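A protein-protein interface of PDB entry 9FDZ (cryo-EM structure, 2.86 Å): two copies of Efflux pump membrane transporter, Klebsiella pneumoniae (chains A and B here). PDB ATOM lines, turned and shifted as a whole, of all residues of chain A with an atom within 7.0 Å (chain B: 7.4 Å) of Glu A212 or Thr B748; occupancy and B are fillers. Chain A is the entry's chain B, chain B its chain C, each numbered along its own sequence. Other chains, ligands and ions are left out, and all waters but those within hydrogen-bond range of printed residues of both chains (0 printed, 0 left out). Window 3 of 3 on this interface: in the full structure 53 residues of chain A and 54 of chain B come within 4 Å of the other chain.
The backbone carbonyl oxygen of Gln A213 lies within hydrogen-bond range of the guanidinium group of Arg B737, at 2.6 Å. The backbone carbonyl oxygen (O) of Gly A241 lies within hydrogen-bond range of the guanidinium group (NH2) of Arg B737 (2.6 Å).
NE2 of Gln A213 sits at hydrogen-bond distance from O of Ile A253, at 2.5 Å. The backbone carbonyl oxygen (O) of Gly A241 is in hydrogen-bond range of the backbone NH (N) of Val A215 (3.5 Å). The side-chain hydroxyl of Ser B746 lies close to the backbone NH of Thr B748 (3.3 Å).
Among the printed residues, pairs that only touch across the chains: Val A215 with Phe B751, Gly A241 with Phe B751, Glu A212 with Thr B748 and Gln A213 with Leu B747.
Glu A212 touches just one residue of chain B: Thr B748 (3.9 Å). Of chain A, only Glu A212 comes within 4 Å of Thr B748. Printed residues of chain A within 4 Å of Leu B747: Gln A213 (3.9 Å). Printed residues of chain B within 4 Å of Gln A213: Arg B737 (2.6 Å) and Leu B747 (3.9 Å). Thr B795 touches none of the printed residues of chain A. The nearest residue of chain B that does not touch Glu A212 is Leu B747 (4.3 Å). The nearest residue of chain A that does not touch Thr B748 is Gln A213 (6.4 Å). The nearest printed residue of chain B that does not touch Val A215 is Arg B737 (5.4 Å).
Hydrophobic or aromatic side chains of chain A that line the printed part of chain B: Val A215. Among the printed residues, no Asp or Glu carboxylate lies within 4 Å of a Lys or Arg side-chain nitrogen of the other chain.
No position is printed for both chains.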
ATOM      1  N   ASP A 205     -21.734  12.533  -9.152  1.00  0.00           N
ATOM      2  CA  ASP A 205     -22.526  13.278 -10.125  1.00  0.00           C
ATOM      3  C   ASP A 205     -23.189  14.490  -9.485  1.00  0.00           C
ATOM      4  O   ASP A 205     -23.229  15.572 -10.080  1.00  0.00           O
ATOM      5  CB  ASP A 205     -23.583  12.371 -10.753  1.00  0.00           C
ATOM      6  CG  ASP A 205     -22.987  11.345 -11.691  1.00  0.00           C
ATOM      7  OD1 ASP A 205     -22.116  11.719 -12.504  1.00  0.00           O
ATOM      8  OD2 ASP A 205     -23.392  10.167 -11.620  1.00  0.00           O
ATOM      9  N   VAL A 207     -22.247  16.102  -6.649  1.00  0.00           N
ATOM     10  CA  VAL A 207     -21.251  17.070  -6.200  1.00  0.00           C
ATOM     11  C   VAL A 207     -20.710  17.867  -7.378  1.00  0.00           C
ATOM     12  O   VAL A 207     -20.520  19.085  -7.287  1.00  0.00           O
ATOM     13  CB  VAL A 207     -20.123  16.359  -5.429  1.00  0.00           C
ATOM     14  CG1 VAL A 207     -18.959  17.303  -5.197  1.00  0.00           C
ATOM     15  CG2 VAL A 207     -20.647  15.831  -4.110  1.00  0.00           C
ATOM     16  N   THR A 208     -20.467  17.197  -8.507  1.00  0.00           N
ATOM     17  CA  THR A 208     -19.965  17.889  -9.689  1.00  0.00           C
ATOM     18  C   THR A 208     -20.960  18.932 -10.183  1.00  0.00           C
ATOM     19  O   THR A 208     -20.571  20.038 -10.573  1.00  0.00           O
ATOM     20  CB  THR A 208     -19.656  16.881 -10.795  1.00  0.00           C
ATOM     21  OG1 THR A 208     -18.587  16.024 -10.377  1.00  0.00           O
ATOM     22  CG2 THR A 208     -19.251  17.592 -12.074  1.00  0.00           C
ATOM     23  N   ALA A 209     -22.252  18.598 -10.166  1.00  0.00           N
ATOM     24  CA  ALA A 209     -23.264  19.529 -10.652  1.00  0.00           C
ATOM     25  C   ALA A 209     -23.319  20.790  -9.801  1.00  0.00           C
ATOM     26  O   ALA A 209     -23.463  21.898 -10.331  1.00  0.00           O
ATOM     27  CB  ALA A 209     -24.629  18.846 -10.687  1.00  0.00           C
ATOM     28  N   MET A 210     -23.214  20.649  -8.478  1.00  0.00           N
ATOM     29  CA  MET A 210     -23.350  21.812  -7.606  1.00  0.00           C
ATOM     30  C   MET A 210     -22.164  22.758  -7.736  1.00  0.00           C
ATOM     31  O   MET A 210     -22.328  23.978  -7.627  1.00  0.00           O
ATOM     32  CB  MET A 210     -23.530  21.375  -6.153  1.00  0.00           C
ATOM     33  CG  MET A 210     -24.534  20.254  -5.958  1.00  0.00           C
ATOM     34  SD  MET A 210     -24.555  19.584  -4.286  1.00  0.00           S
ATOM     35  CE  MET A 210     -23.654  20.847  -3.396  1.00  0.00           C
ATOM     36  N   GLN A 211     -20.964  22.229  -7.959  1.00  0.00           N
ATOM     37  CA  GLN A 211     -19.779  23.074  -8.035  1.00  0.00           C
ATOM     38  C   GLN A 211     -19.557  23.660  -9.421  1.00  0.00           C
ATOM     39  O   GLN A 211     -18.637  24.465  -9.595  1.00  0.00           O
ATOM     40  CB  GLN A 211     -18.533  22.297  -7.597  1.00  0.00           C
ATOM     41  CG  GLN A 211     -18.295  20.998  -8.326  1.00  0.00           C
ATOM     42  CD  GLN A 211     -17.009  20.328  -7.888  1.00  0.00           C
ATOM     43  OE1 GLN A 211     -16.347  20.784  -6.958  1.00  0.00           O
ATOM     44  NE2 GLN A 211     -16.649  19.240  -8.558  1.00  0.00           N
ATOM     45  N   GLU A 212     -20.368  23.282 -10.405  1.00  0.00           N
ATOM     46  CA  GLU A 212     -20.305  23.875 -11.732  1.00  0.00           C
ATOM     47  C   GLU A 212     -21.488  24.783 -12.024  1.00  0.00           C
ATOM     48  O   GLU A 212     -21.501  25.447 -13.064  1.00  0.00           O
ATOM     49  CB  GLU A 212     -20.214  22.781 -12.800  1.00  0.00           C
ATOM     50  CG  GLU A 212     -21.551  22.199 -13.208  1.00  0.00           C
ATOM     51  CD  GLU A 212     -21.407  21.001 -14.121  1.00  0.00           C
ATOM     52  OE1 GLU A 212     -20.257  20.622 -14.426  1.00  0.00           O
ATOM     53  OE2 GLU A 212     -22.442  20.438 -14.535  1.00  0.00           O
ATOM     54  N   GLN A 213     -22.481  24.831 -11.137  1.00  0.00           N
ATOM     55  CA  GLN A 213     -23.620  25.723 -11.280  1.00  0.00           C
ATOM     56  C   GLN A 213     -23.624  26.842 -10.251  1.00  0.00           C
ATOM     57  O   GLN A 213     -24.508  27.703 -10.295  1.00  0.00           O
ATOM     58  CB  GLN A 213     -24.929  24.933 -11.187  1.00  0.00           C
ATOM     59  CG  GLN A 213     -25.120  23.930 -12.303  1.00  0.00           C
ATOM     60  CD  GLN A 213     -26.508  23.334 -12.315  1.00  0.00           C
ATOM     61  OE1 GLN A 213     -27.492  24.024 -12.060  1.00  0.00           O
ATOM     62  NE2 GLN A 213     -26.595  22.043 -12.609  1.00  0.00           N
ATOM     63  N   ASN A 214     -22.667  26.850  -9.325  1.00  0.00           N
ATOM     64  CA  ASN A 214     -22.522  27.905  -8.324  1.00  0.00           C
ATOM     65  C   ASN A 214     -21.064  28.353  -8.375  1.00  0.00           C
ATOM     66  O   ASN A 214     -20.228  27.871  -7.607  1.00  0.00           O
ATOM     67  CB  ASN A 214     -22.923  27.406  -6.939  1.00  0.00           C
ATOM     68  CG  ASN A 214     -22.593  28.396  -5.842  1.00  0.00           C
ATOM     69  OD1 ASN A 214     -23.034  29.542  -5.872  1.00  0.00           O
ATOM     70  ND2 ASN A 214     -21.813  27.958  -4.864  1.00  0.00           N
ATOM     71  N   VAL A 215     -20.763  29.273  -9.286  1.00  0.00           N
ATOM     72  CA  VAL A 215     -19.402  29.744  -9.504  1.00  0.00           C
ATOM     73  C   VAL A 215     -19.404  31.263  -9.547  1.00  0.00           C
ATOM     74  O   VAL A 215     -20.438  31.897  -9.779  1.00  0.00           O
ATOM     75  CB  VAL A 215     -18.793  29.169 -10.800  1.00  0.00           C
ATOM     76  CG1 VAL A 215     -18.593  27.670 -10.676  1.00  0.00           C
ATOM     77  CG2 VAL A 215     -19.677  29.493 -11.986  1.00  0.00           C
ATOM     78  N   GLY A 241     -23.043  34.298 -11.128  1.00  0.00           N
ATOM     79  CA  GLY A 241     -23.318  32.896 -11.363  1.00  0.00           C
ATOM     80  C   GLY A 241     -23.494  32.124 -10.073  1.00  0.00           C
ATOM     81  O   GLY A 241     -23.713  30.910 -10.092  1.00  0.00           O
ATOM     82  N   ILE A 253     -30.052  21.904 -11.372  1.00  0.00           N
ATOM     83  CA  ILE A 253     -30.440  20.835 -12.282  1.00  0.00           C
ATOM     84  C   ILE A 253     -29.354  19.770 -12.280  1.00  0.00           C
ATOM     85  O   ILE A 253     -28.181  20.063 -12.541  1.00  0.00           O
ATOM     86  CB  ILE A 253     -30.675  21.380 -13.700  1.00  0.00           C
ATOM     87  CG1 ILE A 253     -31.745  22.469 -13.676  1.00  0.00           C
ATOM     88  CG2 ILE A 253     -31.081  20.261 -14.635  1.00  0.00           C
ATOM     89  CD1 ILE A 253     -31.656  23.434 -14.833  1.00  0.00           C
ATOM     90  N   LEU A 254     -29.743  18.531 -11.988  1.00  0.00           N
ATOM     91  CA  LEU A 254     -28.811  17.412 -11.949  1.00  0.00           C
ATOM     92  C   LEU A 254     -28.757  16.636 -13.256  1.00  0.00           C
ATOM     93  O   LEU A 254     -27.672  16.249 -13.696  1.00  0.00           O
ATOM     94  CB  LEU A 254     -29.177  16.458 -10.810  1.00  0.00           C
ATOM     95  CG  LEU A 254     -29.145  17.041  -9.399  1.00  0.00           C
ATOM     96  CD1 LEU A 254     -29.435  15.959  -8.379  1.00  0.00           C
ATOM     97  CD2 LEU A 254     -27.809  17.698  -9.118  1.00  0.00           C
ATOM     98  N   VAL A 763     -17.906  21.215  -1.075  1.00  0.00           N
ATOM     99  CA  VAL A 763     -18.128  21.440  -2.499  1.00  0.00           C
ATOM    100  C   VAL A 763     -17.499  22.753  -2.947  1.00  0.00           C
ATOM    101  O   VAL A 763     -16.581  22.760  -3.774  1.00  0.00           O
ATOM    102  CB  VAL A 763     -19.632  21.417  -2.820  1.00  0.00           C
ATOM    103  CG1 VAL A 763     -19.854  21.506  -4.313  1.00  0.00           C
ATOM    104  CG2 VAL A 763     -20.263  20.160  -2.260  1.00  0.00           C
ATOM    105  N   ASN A 764     -17.973  23.863  -2.398  1.00  0.00           N
ATOM    106  CA  ASN A 764     -17.489  25.196  -2.751  1.00  0.00           C
ATOM    107  C   ASN A 764     -18.055  26.179  -1.730  1.00  0.00           C
ATOM    108  O   ASN A 764     -18.595  25.776  -0.694  1.00  0.00           O
ATOM    109  CB  ASN A 764     -17.863  25.568  -4.186  1.00  0.00           C
ATOM    110  CG  ASN A 764     -19.335  25.376  -4.476  1.00  0.00           C
ATOM    111  OD1 ASN A 764     -20.101  24.959  -3.610  1.00  0.00           O
ATOM    112  ND2 ASN A 764     -19.737  25.674  -5.702  1.00  0.00           N
ATOM    113  N   SER B 204     -12.756  28.985 -24.012  1.00  0.00           N
ATOM    114  CA  SER B 204     -12.106  27.960 -23.201  1.00  0.00           C
ATOM    115  C   SER B 204     -11.123  27.142 -24.029  1.00  0.00           C
ATOM    116  O   SER B 204     -10.048  26.771 -23.542  1.00  0.00           O
ATOM    117  CB  SER B 204     -13.157  27.053 -22.564  1.00  0.00           C
ATOM    118  OG  SER B 204     -14.234  27.810 -22.040  1.00  0.00           O
ATOM    119  N   ARG B 737     -30.996  30.241 -16.156  1.00  0.00           N
ATOM    120  CA  ARG B 737     -30.525  28.860 -16.132  1.00  0.00           C
ATOM    121  C   ARG B 737     -31.486  27.918 -16.845  1.00  0.00           C
ATOM    122  O   ARG B 737     -31.051  26.923 -17.435  1.00  0.00           O
ATOM    123  CB  ARG B 737     -30.309  28.412 -14.689  1.00  0.00           C
ATOM    124  CG  ARG B 737     -29.059  28.989 -14.046  1.00  0.00           C
ATOM    125  CD  ARG B 737     -28.830  28.394 -12.670  1.00  0.00           C
ATOM    126  NE  ARG B 737     -27.467  28.599 -12.195  1.00  0.00           N
ATOM    127  CZ  ARG B 737     -27.016  29.735 -11.684  1.00  0.00           C
ATOM    128  NH1 ARG B 737     -27.791  30.801 -11.574  1.00  0.00           N
ATOM    129  NH2 ARG B 737     -25.755  29.803 -11.271  1.00  0.00           N
ATOM    130  N   VAL B 745     -26.952  24.500 -23.861  1.00  0.00           N
ATOM    131  CA  VAL B 745     -25.667  25.147 -23.626  1.00  0.00           C
ATOM    132  C   VAL B 745     -25.257  24.890 -22.185  1.00  0.00           C
ATOM    133  O   VAL B 745     -26.007  25.204 -21.254  1.00  0.00           O
ATOM    134  CB  VAL B 745     -25.731  26.655 -23.918  1.00  0.00           C
ATOM    135  CG1 VAL B 745     -24.445  27.332 -23.480  1.00  0.00           C
ATOM    136  CG2 VAL B 745     -25.988  26.897 -25.394  1.00  0.00           C
ATOM    137  N   SER B 746     -24.070  24.318 -22.003  1.00  0.00           N
ATOM    138  CA  SER B 746     -23.562  24.054 -20.665  1.00  0.00           C
ATOM    139  C   SER B 746     -23.237  25.362 -19.957  1.00  0.00           C
ATOM    140  O   SER B 746     -22.717  26.298 -20.569  1.00  0.00           O
ATOM    141  CB  SER B 746     -22.320  23.169 -20.738  1.00  0.00           C
ATOM    142  OG  SER B 746     -21.760  22.970 -19.452  1.00  0.00           O
ATOM    143  N   LEU B 747     -23.548  25.426 -18.660  1.00  0.00           N
ATOM    144  CA  LEU B 747     -23.231  26.625 -17.892  1.00  0.00           C
ATOM    145  C   LEU B 747     -21.728  26.811 -17.745  1.00  0.00           C
ATOM    146  O   LEU B 747     -21.258  27.942 -17.585  1.00  0.00           O
ATOM    147  CB  LEU B 747     -23.894  26.565 -16.517  1.00  0.00           C
ATOM    148  CG  LEU B 747     -25.380  26.916 -16.480  1.00  0.00           C
ATOM    149  CD1 LEU B 747     -25.981  26.535 -15.141  1.00  0.00           C
ATOM    150  CD2 LEU B 747     -25.585  28.393 -16.759  1.00  0.00           C
ATOM    151  N   THR B 748     -20.961  25.720 -17.791  1.00  0.00           N
ATOM    152  CA  THR B 748     -19.509  25.839 -17.732  1.00  0.00           C
ATOM    153  C   THR B 748     -18.975  26.613 -18.929  1.00  0.00           C
ATOM    154  O   THR B 748     -18.087  27.463 -18.785  1.00  0.00           O
ATOM    155  CB  THR B 748     -18.869  24.454 -17.664  1.00  0.00           C
ATOM    156  OG1 THR B 748     -19.507  23.679 -16.643  1.00  0.00           O
ATOM    157  CG2 THR B 748     -17.386  24.568 -17.353  1.00  0.00           C
ATOM    158  N   GLU B 749     -19.503  26.334 -20.122  1.00  0.00           N
ATOM    159  CA  GLU B 749     -19.070  27.063 -21.308  1.00  0.00           C
ATOM    160  C   GLU B 749     -19.641  28.475 -21.330  1.00  0.00           C
ATOM    161  O   GLU B 749     -18.954  29.421 -21.731  1.00  0.00           O
ATOM    162  CB  GLU B 749     -19.473  26.299 -22.568  1.00  0.00           C
ATOM    163  CG  GLU B 749     -18.497  25.207 -22.974  1.00  0.00           C
ATOM    164  CD  GLU B 749     -17.126  25.750 -23.330  1.00  0.00           C
ATOM    165  OE1 GLU B 749     -16.275  25.870 -22.423  1.00  0.00           O
ATOM    166  OE2 GLU B 749     -16.898  26.060 -24.518  1.00  0.00           O
ATOM    167  N   LEU B 750     -20.897  28.637 -20.909  1.00  0.00           N
ATOM    168  CA  LEU B 750     -21.510  29.961 -20.904  1.00  0.00           C
ATOM    169  C   LEU B 750     -20.802  30.895 -19.931  1.00  0.00           C
ATOM    170  O   LEU B 750     -20.547  32.061 -20.252  1.00  0.00           O
ATOM    171  CB  LEU B 750     -22.994  29.851 -20.560  1.00  0.00           C
ATOM    172  CG  LEU B 750     -23.754  31.164 -20.367  1.00  0.00           C
ATOM    173  CD1 LEU B 750     -23.580  32.071 -21.571  1.00  0.00           C
ATOM    174  CD2 LEU B 750     -25.224  30.892 -20.113  1.00  0.00           C
ATOM    175  N   PHE B 751     -20.479  30.405 -18.733  1.00  0.00           N
ATOM    176  CA  PHE B 751     -19.733  31.223 -17.785  1.00  0.00           C
ATOM    177  C   PHE B 751     -18.300  31.436 -18.252  1.00  0.00           C
ATOM    178  O   PHE B 751     -17.719  32.502 -18.023  1.00  0.00           O
ATOM    179  CB  PHE B 751     -19.758  30.582 -16.398  1.00  0.00           C
ATOM    180  CG  PHE B 751     -21.089  30.674 -15.711  1.00  0.00           C
ATOM    181  CD1 PHE B 751     -21.847  31.828 -15.794  1.00  0.00           C
ATOM    182  CD2 PHE B 751     -21.580  29.609 -14.977  1.00  0.00           C
ATOM    183  CE1 PHE B 751     -23.071  31.916 -15.163  1.00  0.00           C
ATOM    184  CE2 PHE B 751     -22.804  29.692 -14.344  1.00  0.00           C
ATOM    185  CZ  PHE B 751     -23.549  30.846 -14.438  1.00  0.00           C
ATOM    186  N   GLY B 752     -17.713  30.431 -18.904  1.00  0.00           N
ATOM    187  CA  GLY B 752     -16.363  30.581 -19.418  1.00  0.00           C
ATOM    188  C   GLY B 752     -16.254  31.628 -20.508  1.00  0.00           C
ATOM    189  O   GLY B 752     -15.224  32.294 -20.631  1.00  0.00           O
ATOM    190  N   THR B 753     -17.302  31.777 -21.319  1.00  0.00           N
ATOM    191  CA  THR B 753     -17.301  32.806 -22.354  1.00  0.00           C
ATOM    192  C   THR B 753     -17.267  34.200 -21.739  1.00  0.00           C
ATOM    193  O   THR B 753     -16.478  35.057 -22.155  1.00  0.00           O
ATOM    194  CB  THR B 753     -18.527  32.642 -23.251  1.00  0.00           C
ATOM    195  OG1 THR B 753     -18.439  31.398 -23.956  1.00  0.00           O
ATOM    196  CG2 THR B 753     -18.616  33.778 -24.250  1.00  0.00           C
ATOM    197  N   LEU B 754     -18.116  34.445 -20.740  1.00  0.00           N
ATOM    198  CA  LEU B 754     -18.113  35.740 -20.068  1.00  0.00           C
ATOM    199  C   LEU B 754     -16.824  35.952 -19.286  1.00  0.00           C
ATOM    200  O   LEU B 754     -16.280  37.062 -19.259  1.00  0.00           O
ATOM    201  CB  LEU B 754     -19.322  35.852 -19.141  1.00  0.00           C
ATOM    202  CG  LEU B 754     -20.701  35.807 -19.796  1.00  0.00           C
ATOM    203  CD1 LEU B 754     -21.772  35.549 -18.753  1.00  0.00           C
ATOM    204  CD2 LEU B 754     -20.977  37.100 -20.534  1.00  0.00           C
ATOM    205  N   GLN B 755     -16.321  34.899 -18.641  1.00  0.00           N
ATOM    206  CA  GLN B 755     -15.143  35.038 -17.794  1.00  0.00           C
ATOM    207  C   GLN B 755     -13.895  35.363 -18.603  1.00  0.00           C
ATOM    208  O   GLN B 755     -13.010  36.074 -18.114  1.00  0.00           O
ATOM    209  CB  GLN B 755     -14.935  33.759 -16.982  1.00  0.00           C
ATOM    210  CG  GLN B 755     -13.614  33.686 -16.236  1.00  0.00           C
ATOM    211  CD  GLN B 755     -13.451  34.804 -15.230  1.00  0.00           C
ATOM    212  OE1 GLN B 755     -13.991  34.745 -14.127  1.00  0.00           O
ATOM    213  NE2 GLN B 755     -12.697  35.829 -15.604  1.00  0.00           N
ATOM    214  N   THR B 795     -21.127  30.843 -28.010  1.00  0.00           N
ATOM    215  CA  THR B 795     -20.723  29.707 -27.198  1.00  0.00           C
ATOM    216  C   THR B 795     -21.217  28.422 -27.848  1.00  0.00           C
ATOM    217  O   THR B 795     -22.287  28.392 -28.462  1.00  0.00           O
ATOM    218  CB  THR B 795     -21.275  29.818 -25.768  1.00  0.00           C
ATOM    219  OG1 THR B 795     -20.987  31.121 -25.247  1.00  0.00           O
ATOM    220  CG2 THR B 795     -20.640  28.782 -24.865  1.00  0.00           C
